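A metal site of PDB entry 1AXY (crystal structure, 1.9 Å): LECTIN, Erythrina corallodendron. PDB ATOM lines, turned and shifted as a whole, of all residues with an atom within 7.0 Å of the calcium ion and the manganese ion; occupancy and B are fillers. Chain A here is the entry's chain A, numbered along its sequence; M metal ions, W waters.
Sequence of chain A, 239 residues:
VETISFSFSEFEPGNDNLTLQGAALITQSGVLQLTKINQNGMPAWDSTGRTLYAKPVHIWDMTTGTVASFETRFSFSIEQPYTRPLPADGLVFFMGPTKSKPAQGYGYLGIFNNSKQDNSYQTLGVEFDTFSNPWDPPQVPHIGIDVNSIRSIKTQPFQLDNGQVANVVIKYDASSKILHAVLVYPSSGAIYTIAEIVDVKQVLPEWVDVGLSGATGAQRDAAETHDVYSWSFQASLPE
The backbone NH (N) of Glu 127 lies within hydrogen-bond range of the backbone carbonyl oxygen (O) of Gly 144 (2.8 Å).
The manganese ion is bound by OD1 of Asp 136 (2.4 Å).
The side-chain carboxylate (OD2) of Asp 129 is bound to the manganese ion (2.4 Å).
Water W3 is bound to the manganese ion, 2.4 Å away.
NE2 of His 142 is bound to the manganese ion (2.5 Å).
The manganese ion is bound by water W1 (2.5 Å).
The manganese ion is bound by OE2 of Glu 127 (2.5 Å).
The manganese ion has six donor atoms within binding distance.
Of the 26 residues printed, 4 come within 4 Å of the manganese ion.
Along chain A the residues within 4 Å of the manganese ion span positions 127 to 142.
Within 4 Å of the calcium ion: Asp 129, Phe 131, Asn 133 and Asp 136.
The calcium ion is bound by the side-chain carboxylate (OD2) of Asp 136 (2.4 Å), the side-chain carboxylate (OD2) of Asp 129 (2.4 Å), the side-chain amide oxygen (OD1) of Asn 133 (2.4 Å), water W2 (2.4 Å), the backbone carbonyl oxygen (O) of Phe 131 (2.4 Å), water W4 (2.5 Å) and the side-chain carboxylate (OD1) of Asp 129 (2.6 Å).
Water W4 bridges the backbone carbonyl oxygen (O) of Gly 107 and the indole nitrogen (NE1) of Trp 135.
Water W1 lies within hydrogen-bond range of the side-chain carboxylate (OE1) of Glu 127 (2.5 Å), the backbone carbonyl oxygen (O) of Ile 150 (2.6 Å) and the indole nitrogen (NE1) of Trp 135 (3.4 Å).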
ATOM      1  N   ASP A  89       9.231 -20.252 -23.976  1.00  0.00           N
ATOM      2  CA  ASP A  89       7.951 -20.692 -24.513  1.00  0.00           C
ATOM      3  C   ASP A  89       6.843 -19.648 -24.275  1.00  0.00           C
ATOM      4  O   ASP A  89       5.835 -19.624 -25.011  1.00  0.00           O
ATOM      5  CB  ASP A  89       7.529 -22.006 -23.868  1.00  0.00           C
ATOM      6  CG  ASP A  89       7.908 -23.205 -24.719  1.00  0.00           C
ATOM      7  OD1 ASP A  89       7.210 -23.473 -25.714  1.00  0.00           O
ATOM      8  OD2 ASP A  89       8.904 -23.885 -24.393  1.00  0.00           O
ATOM      9  N   GLY A  90       7.014 -18.825 -23.251  1.00  0.00           N
ATOM     10  CA  GLY A  90       6.039 -17.794 -22.951  1.00  0.00           C
ATOM     11  C   GLY A  90       5.666 -17.713 -21.486  1.00  0.00           C
ATOM     12  O   GLY A  90       6.281 -18.367 -20.655  1.00  0.00           O
ATOM     13  N   TYR A 106       7.692 -26.069 -20.762  1.00  0.00           N
ATOM     14  CA  TYR A 106       7.721 -25.857 -22.199  1.00  0.00           C
ATOM     15  C   TYR A 106       6.412 -25.222 -22.671  1.00  0.00           C
ATOM     16  O   TYR A 106       5.867 -24.345 -21.997  1.00  0.00           O
ATOM     17  CB  TYR A 106       8.010 -27.173 -22.943  1.00  0.00           C
ATOM     18  CG  TYR A 106       9.144 -27.964 -22.326  1.00  0.00           C
ATOM     19  CD1 TYR A 106      10.357 -27.360 -22.039  1.00  0.00           C
ATOM     20  CD2 TYR A 106       8.972 -29.302 -21.998  1.00  0.00           C
ATOM     21  CE1 TYR A 106      11.381 -28.070 -21.422  1.00  0.00           C
ATOM     22  CE2 TYR A 106       9.974 -30.016 -21.382  1.00  0.00           C
ATOM     23  CZ  TYR A 106      11.182 -29.404 -21.104  1.00  0.00           C
ATOM     24  OH  TYR A 106      12.192 -30.112 -20.498  1.00  0.00           O
ATOM     25  N   GLY A 107       5.906 -25.708 -23.806  1.00  0.00           N
ATOM     26  CA  GLY A 107       4.675 -25.190 -24.378  1.00  0.00           C
ATOM     27  C   GLY A 107       3.441 -25.338 -23.519  1.00  0.00           C
ATOM     28  O   GLY A 107       2.396 -24.793 -23.868  1.00  0.00           O
ATOM     29  N   TYR A 108       3.535 -26.106 -22.438  1.00  0.00           N
ATOM     30  CA  TYR A 108       2.382 -26.281 -21.539  1.00  0.00           C
ATOM     31  C   TYR A 108       2.352 -25.171 -20.503  1.00  0.00           C
ATOM     32  O   TYR A 108       1.443 -25.102 -19.687  1.00  0.00           O
ATOM     33  CB  TYR A 108       2.399 -27.666 -20.898  1.00  0.00           C
ATOM     34  CG  TYR A 108       2.310 -28.765 -21.935  1.00  0.00           C
ATOM     35  CD1 TYR A 108       1.193 -28.859 -22.774  1.00  0.00           C
ATOM     36  CD2 TYR A 108       3.346 -29.664 -22.122  1.00  0.00           C
ATOM     37  CE1 TYR A 108       1.121 -29.833 -23.769  1.00  0.00           C
ATOM     38  CE2 TYR A 108       3.290 -30.626 -23.116  1.00  0.00           C
ATOM     39  CZ  TYR A 108       2.174 -30.706 -23.935  1.00  0.00           C
ATOM     40  OH  TYR A 108       2.132 -31.670 -24.920  1.00  0.00           O
ATOM     41  N   LEU A 109       3.384 -24.328 -20.545  1.00  0.00           N
ATOM     42  CA  LEU A 109       3.522 -23.154 -19.696  1.00  0.00           C
ATOM     43  C   LEU A 109       3.460 -23.341 -18.190  1.00  0.00           C
ATOM     44  O   LEU A 109       3.226 -22.383 -17.450  1.00  0.00           O
ATOM     45  CB  LEU A 109       2.507 -22.076 -20.157  1.00  0.00           C
ATOM     46  CG  LEU A 109       2.574 -21.711 -21.641  1.00  0.00           C
ATOM     47  CD1 LEU A 109       1.447 -20.754 -22.026  1.00  0.00           C
ATOM     48  CD2 LEU A 109       3.920 -21.095 -21.981  1.00  0.00           C
ATOM     49  N   GLU A 127      -2.656 -16.454 -21.919  1.00  0.00           N
ATOM     50  CA  GLU A 127      -1.272 -16.657 -22.310  1.00  0.00           C
ATOM     51  C   GLU A 127      -0.686 -15.619 -23.247  1.00  0.00           C
ATOM     52  O   GLU A 127      -1.398 -14.938 -23.999  1.00  0.00           O
ATOM     53  CB  GLU A 127      -1.107 -18.028 -22.947  1.00  0.00           C
ATOM     54  CG  GLU A 127      -2.123 -18.283 -24.047  1.00  0.00           C
ATOM     55  CD  GLU A 127      -1.641 -19.244 -25.114  1.00  0.00           C
ATOM     56  OE1 GLU A 127      -1.472 -20.452 -24.858  1.00  0.00           O
ATOM     57  OE2 GLU A 127      -1.430 -18.784 -26.244  1.00  0.00           O
ATOM     58  N   PHE A 128       0.644 -15.514 -23.184  1.00  0.00           N
ATOM     59  CA  PHE A 128       1.468 -14.649 -24.009  1.00  0.00           C
ATOM     60  C   PHE A 128       2.514 -15.652 -24.507  1.00  0.00           C
ATOM     61  O   PHE A 128       3.560 -15.872 -23.904  1.00  0.00           O
ATOM     62  CB  PHE A 128       2.031 -13.509 -23.164  1.00  0.00           C
ATOM     63  CG  PHE A 128       0.956 -12.640 -22.589  1.00  0.00           C
ATOM     64  CD1 PHE A 128       0.446 -11.559 -23.322  1.00  0.00           C
ATOM     65  CD2 PHE A 128       0.364 -12.959 -21.372  1.00  0.00           C
ATOM     66  CE1 PHE A 128      -0.647 -10.828 -22.858  1.00  0.00           C
ATOM     67  CE2 PHE A 128      -0.721 -12.222 -20.889  1.00  0.00           C
ATOM     68  CZ  PHE A 128      -1.234 -11.156 -21.642  1.00  0.00           C
ATOM     69  N   ASP A 129       2.082 -16.358 -25.544  1.00  0.00           N
ATOM     70  CA  ASP A 129       2.812 -17.433 -26.188  1.00  0.00           C
ATOM     71  C   ASP A 129       3.807 -16.989 -27.266  1.00  0.00           C
ATOM     72  O   ASP A 129       3.431 -16.431 -28.285  1.00  0.00           O
ATOM     73  CB  ASP A 129       1.788 -18.381 -26.778  1.00  0.00           C
ATOM     74  CG  ASP A 129       2.352 -19.731 -27.088  1.00  0.00           C
ATOM     75  OD1 ASP A 129       3.580 -19.901 -27.221  1.00  0.00           O
ATOM     76  OD2 ASP A 129       1.553 -20.663 -27.184  1.00  0.00           O
ATOM     77  N   THR A 130       5.069 -17.384 -27.072  1.00  0.00           N
ATOM     78  CA  THR A 130       6.145 -17.004 -27.980  1.00  0.00           C
ATOM     79  C   THR A 130       6.661 -18.101 -28.917  1.00  0.00           C
ATOM     80  O   THR A 130       7.514 -17.826 -29.770  1.00  0.00           O
ATOM     81  CB  THR A 130       7.354 -16.480 -27.173  1.00  0.00           C
ATOM     82  OG1 THR A 130       7.786 -17.494 -26.260  1.00  0.00           O
ATOM     83  CG2 THR A 130       6.970 -15.221 -26.401  1.00  0.00           C
ATOM     84  N   PHE A 131       6.178 -19.334 -28.752  1.00  0.00           N
ATOM     85  CA  PHE A 131       6.622 -20.436 -29.591  1.00  0.00           C
ATOM     86  C   PHE A 131       5.428 -21.173 -30.181  1.00  0.00           C
ATOM     87  O   PHE A 131       4.502 -21.528 -29.480  1.00  0.00           O
ATOM     88  CB  PHE A 131       7.482 -21.418 -28.791  1.00  0.00           C
ATOM     89  CG  PHE A 131       7.956 -22.596 -29.591  1.00  0.00           C
ATOM     90  CD1 PHE A 131       9.082 -22.504 -30.402  1.00  0.00           C
ATOM     91  CD2 PHE A 131       7.277 -23.813 -29.529  1.00  0.00           C
ATOM     92  CE1 PHE A 131       9.520 -23.585 -31.150  1.00  0.00           C
ATOM     93  CE2 PHE A 131       7.705 -24.914 -30.268  1.00  0.00           C
ATOM     94  CZ  PHE A 131       8.826 -24.800 -31.078  1.00  0.00           C
ATOM     95  N   SER A 132       5.472 -21.437 -31.484  1.00  0.00           N
ATOM     96  CA  SER A 132       4.366 -22.122 -32.151  1.00  0.00           C
ATOM     97  C   SER A 132       4.420 -23.653 -32.092  1.00  0.00           C
ATOM     98  O   SER A 132       5.216 -24.280 -32.788  1.00  0.00           O
ATOM     99  CB  SER A 132       4.262 -21.647 -33.596  1.00  0.00           C
ATOM    100  OG  SER A 132       3.032 -22.051 -34.172  1.00  0.00           O
ATOM    101  N   ASN A 133       3.580 -24.231 -31.233  1.00  0.00           N
ATOM    102  CA  ASN A 133       3.464 -25.689 -31.076  1.00  0.00           C
ATOM    103  C   ASN A 133       2.435 -26.179 -32.109  1.00  0.00           C
ATOM    104  O   ASN A 133       1.760 -25.383 -32.748  1.00  0.00           O
ATOM    105  CB  ASN A 133       2.995 -26.029 -29.657  1.00  0.00           C
ATOM    106  CG  ASN A 133       4.021 -25.704 -28.596  1.00  0.00           C
ATOM    107  OD1 ASN A 133       4.006 -24.632 -28.001  1.00  0.00           O
ATOM    108  ND2 ASN A 133       4.904 -26.630 -28.336  1.00  0.00           N
ATOM    109  N   PRO A 134       2.307 -27.508 -32.280  1.00  0.00           N
ATOM    110  CA  PRO A 134       1.340 -28.001 -33.262  1.00  0.00           C
ATOM    111  C   PRO A 134      -0.109 -27.672 -32.970  1.00  0.00           C
ATOM    112  O   PRO A 134      -0.944 -27.743 -33.855  1.00  0.00           O
ATOM    113  CB  PRO A 134       1.605 -29.512 -33.279  1.00  0.00           C
ATOM    114  CG  PRO A 134       2.139 -29.790 -31.945  1.00  0.00           C
ATOM    115  CD  PRO A 134       3.080 -28.617 -31.713  1.00  0.00           C
ATOM    116  N   TRP A 135      -0.408 -27.299 -31.729  1.00  0.00           N
ATOM    117  CA  TRP A 135      -1.764 -26.914 -31.345  1.00  0.00           C
ATOM    118  C   TRP A 135      -1.983 -25.393 -31.447  1.00  0.00           C
ATOM    119  O   TRP A 135      -3.086 -24.893 -31.208  1.00  0.00           O
ATOM    120  CB  TRP A 135      -2.074 -27.385 -29.927  1.00  0.00           C
ATOM    121  CG  TRP A 135      -1.098 -26.872 -28.914  1.00  0.00           C
ATOM    122  CD1 TRP A 135      -1.050 -25.616 -28.385  1.00  0.00           C
ATOM    123  CD2 TRP A 135      -0.042 -27.609 -28.297  1.00  0.00           C
ATOM    124  NE1 TRP A 135      -0.026 -25.516 -27.477  1.00  0.00           N
ATOM    125  CE2 TRP A 135       0.603 -26.732 -27.395  1.00  0.00           C
ATOM    126  CE3 TRP A 135       0.417 -28.925 -28.409  1.00  0.00           C
ATOM    127  CZ2 TRP A 135       1.691 -27.132 -26.613  1.00  0.00           C
ATOM    128  CZ3 TRP A 135       1.499 -29.318 -27.627  1.00  0.00           C
ATOM    129  CH2 TRP A 135       2.119 -28.422 -26.744  1.00  0.00           C
ATOM    130  N   ASP A 136      -0.937 -24.675 -31.831  1.00  0.00           N
ATOM    131  CA  ASP A 136      -0.972 -23.217 -31.961  1.00  0.00           C
ATOM    132  C   ASP A 136      -1.170 -22.701 -33.357  1.00  0.00           C
ATOM    133  O   ASP A 136      -0.909 -23.402 -34.343  1.00  0.00           O
ATOM    134  CB  ASP A 136       0.366 -22.634 -31.521  1.00  0.00           C
ATOM    135  CG  ASP A 136       0.527 -22.617 -30.048  1.00  0.00           C
ATOM    136  OD1 ASP A 136      -0.483 -22.424 -29.371  1.00  0.00           O
ATOM    137  OD2 ASP A 136       1.650 -22.804 -29.553  1.00  0.00           O
ATOM    138  N   PRO A 137      -1.658 -21.455 -33.477  1.00  0.00           N
ATOM    139  CA  PRO A 137      -1.847 -20.870 -34.812  1.00  0.00           C
ATOM    140  C   PRO A 137      -0.395 -20.610 -35.235  1.00  0.00           C
ATOM    141  O   PRO A 137       0.506 -20.577 -34.391  1.00  0.00           O
ATOM    142  CB  PRO A 137      -2.589 -19.565 -34.505  1.00  0.00           C
ATOM    143  CG  PRO A 137      -2.204 -19.245 -33.084  1.00  0.00           C
ATOM    144  CD  PRO A 137      -2.263 -20.612 -32.434  1.00  0.00           C
ATOM    145  N   VAL A 140       3.302 -16.089 -34.023  1.00  0.00           N
ATOM    146  CA  VAL A 140       3.804 -15.906 -32.662  1.00  0.00           C
ATOM    147  C   VAL A 140       4.594 -14.607 -32.671  1.00  0.00           C
ATOM    148  O   VAL A 140       5.204 -14.250 -33.677  1.00  0.00           O
ATOM    149  CB  VAL A 140       4.712 -17.076 -32.164  1.00  0.00           C
ATOM    150  CG1 VAL A 140       3.881 -18.269 -31.764  1.00  0.00           C
ATOM    151  CG2 VAL A 140       5.713 -17.463 -33.234  1.00  0.00           C
ATOM    152  N   HIS A 142       1.534 -14.524 -29.588  1.00  0.00           N
ATOM    153  CA  HIS A 142       0.092 -14.314 -29.567  1.00  0.00           C
ATOM    154  C   HIS A 142      -0.474 -14.390 -28.167  1.00  0.00           C
ATOM    155  O   HIS A 142       0.098 -15.038 -27.287  1.00  0.00           O
ATOM    156  CB  HIS A 142      -0.659 -15.282 -30.493  1.00  0.00           C
ATOM    157  CG  HIS A 142      -0.467 -16.724 -30.161  1.00  0.00           C
ATOM    158  ND1 HIS A 142       0.428 -17.552 -30.808  1.00  0.00           N
ATOM    159  CD2 HIS A 142      -1.073 -17.501 -29.221  1.00  0.00           C
ATOM    160  CE1 HIS A 142       0.343 -18.763 -30.257  1.00  0.00           C
ATOM    161  NE2 HIS A 142      -0.552 -18.784 -29.291  1.00  0.00           N
ATOM    162  N   ILE A 143      -1.539 -13.637 -27.953  1.00  0.00           N
ATOM    163  CA  ILE A 143      -2.251 -13.647 -26.694  1.00  0.00           C
ATOM    164  C   ILE A 143      -3.302 -14.741 -26.886  1.00  0.00           C
ATOM    165  O   ILE A 143      -3.833 -14.909 -27.997  1.00  0.00           O
ATOM    166  CB  ILE A 143      -3.018 -12.324 -26.458  1.00  0.00           C
ATOM    167  CG1 ILE A 143      -2.081 -11.114 -26.616  1.00  0.00           C
ATOM    168  CG2 ILE A 143      -3.644 -12.319 -25.067  1.00  0.00           C
ATOM    169  CD1 ILE A 143      -2.802  -9.793 -26.649  1.00  0.00           C
ATOM    170  N   GLY A 144      -3.573 -15.518 -25.861  1.00  0.00           N
ATOM    171  CA  GLY A 144      -4.586 -16.547 -26.012  1.00  0.00           C
ATOM    172  C   GLY A 144      -5.389 -16.736 -24.747  1.00  0.00           C
ATOM    173  O   GLY A 144      -4.879 -16.522 -23.656  1.00  0.00           O
ATOM    174  N   ASP A 146      -7.134 -19.426 -22.592  1.00  0.00           N
ATOM    175  CA  ASP A 146      -7.135 -20.873 -22.373  1.00  0.00           C
ATOM    176  C   ASP A 146      -8.190 -21.300 -21.375  1.00  0.00           C
ATOM    177  O   ASP A 146      -8.214 -20.822 -20.248  1.00  0.00           O
ATOM    178  CB  ASP A 146      -5.758 -21.333 -21.867  1.00  0.00           C
ATOM    179  CG  ASP A 146      -4.618 -20.955 -22.804  1.00  0.00           C
ATOM    180  OD1 ASP A 146      -4.893 -20.546 -23.943  1.00  0.00           O
ATOM    181  OD2 ASP A 146      -3.451 -21.047 -22.397  1.00  0.00           O
ATOM    182  N   ILE A 150      -4.510 -26.073 -23.325  1.00  0.00           N
ATOM    183  CA  ILE A 150      -3.474 -25.200 -23.856  1.00  0.00           C
ATOM    184  C   ILE A 150      -3.888 -24.745 -25.277  1.00  0.00           C
ATOM    185  O   ILE A 150      -3.296 -23.829 -25.845  1.00  0.00           O
ATOM    186  CB  ILE A 150      -2.087 -25.925 -23.855  1.00  0.00           C
ATOM    187  CG1 ILE A 150      -0.951 -24.929 -24.123  1.00  0.00           C
ATOM    188  CG2 ILE A 150      -2.073 -27.097 -24.841  1.00  0.00           C
ATOM    189  CD1 ILE A 150      -0.770 -23.887 -23.025  1.00  0.00           C
ATOM    190  N   ARG A 151      -4.904 -25.388 -25.832  1.00  0.00           N
ATOM    191  CA  ARG A 151      -5.434 -25.031 -27.156  1.00  0.00           C
ATOM    192  C   ARG A 151      -6.430 -23.903 -26.935  1.00  0.00           C
ATOM    193  O   ARG A 151      -7.607 -24.157 -26.657  1.00  0.00           O
ATOM    194  CB  ARG A 151      -6.171 -26.214 -27.774  1.00  0.00           C
ATOM    195  CG  ARG A 151      -5.383 -27.485 -27.910  1.00  0.00           C
ATOM    196  CD  ARG A 151      -6.152 -28.430 -28.795  1.00  0.00           C
ATOM    197  NE  ARG A 151      -6.465 -29.674 -28.118  1.00  0.00           N
ATOM    198  CZ  ARG A 151      -7.693 -30.190 -28.004  1.00  0.00           C
ATOM    199  NH1 ARG A 151      -8.747 -29.577 -28.532  1.00  0.00           N
ATOM    200  NH2 ARG A 151      -7.838 -31.372 -27.433  1.00  0.00           N
ATOM    201  N   SER A 152      -5.981 -22.658 -27.101  1.00  0.00           N
ATOM    202  CA  SER A 152      -6.826 -21.480 -26.877  1.00  0.00           C
ATOM    203  C   SER A 152      -8.147 -21.489 -27.628  1.00  0.00           C
ATOM    204  O   SER A 152      -8.225 -21.981 -28.737  1.00  0.00           O
ATOM    205  CB  SER A 152      -6.077 -20.211 -27.268  1.00  0.00           C
ATOM    206  OG  SER A 152      -4.784 -20.209 -26.687  1.00  0.00           O
ATOM    207  N   THR A 155      -7.431 -16.486 -30.067  1.00  0.00           N
ATOM    208  CA  THR A 155      -6.046 -16.065 -30.159  1.00  0.00           C
ATOM    209  C   THR A 155      -5.928 -14.692 -30.828  1.00  0.00           C
ATOM    210  O   THR A 155      -6.770 -14.320 -31.626  1.00  0.00           O
ATOM    211  CB  THR A 155      -5.243 -17.149 -30.952  1.00  0.00           C
ATOM    212  OG1 THR A 155      -4.413 -17.893 -30.049  1.00  0.00           O
ATOM    213  CG2 THR A 155      -4.413 -16.566 -32.051  1.00  0.00           C
HETATM  214 CA    CA M   1       3.119 -22.413 -27.694  1.00  0.00          CA
HETATM  215 MN    MN M   2      -0.787 -20.683 -27.751  1.00  0.00          MN
HETATM  216  O   HOH W   1      -1.086 -22.581 -26.182  1.00  0.00           O
HETATM  217  O   HOH W   2       4.952 -22.149 -26.151  1.00  0.00           O
HETATM  218  O   HOH W   3      -3.059 -20.802 -28.579  1.00  0.00           O
HETATM  219  O   HOH W   4       1.619 -23.372 -26.001  1.00  0.00           O
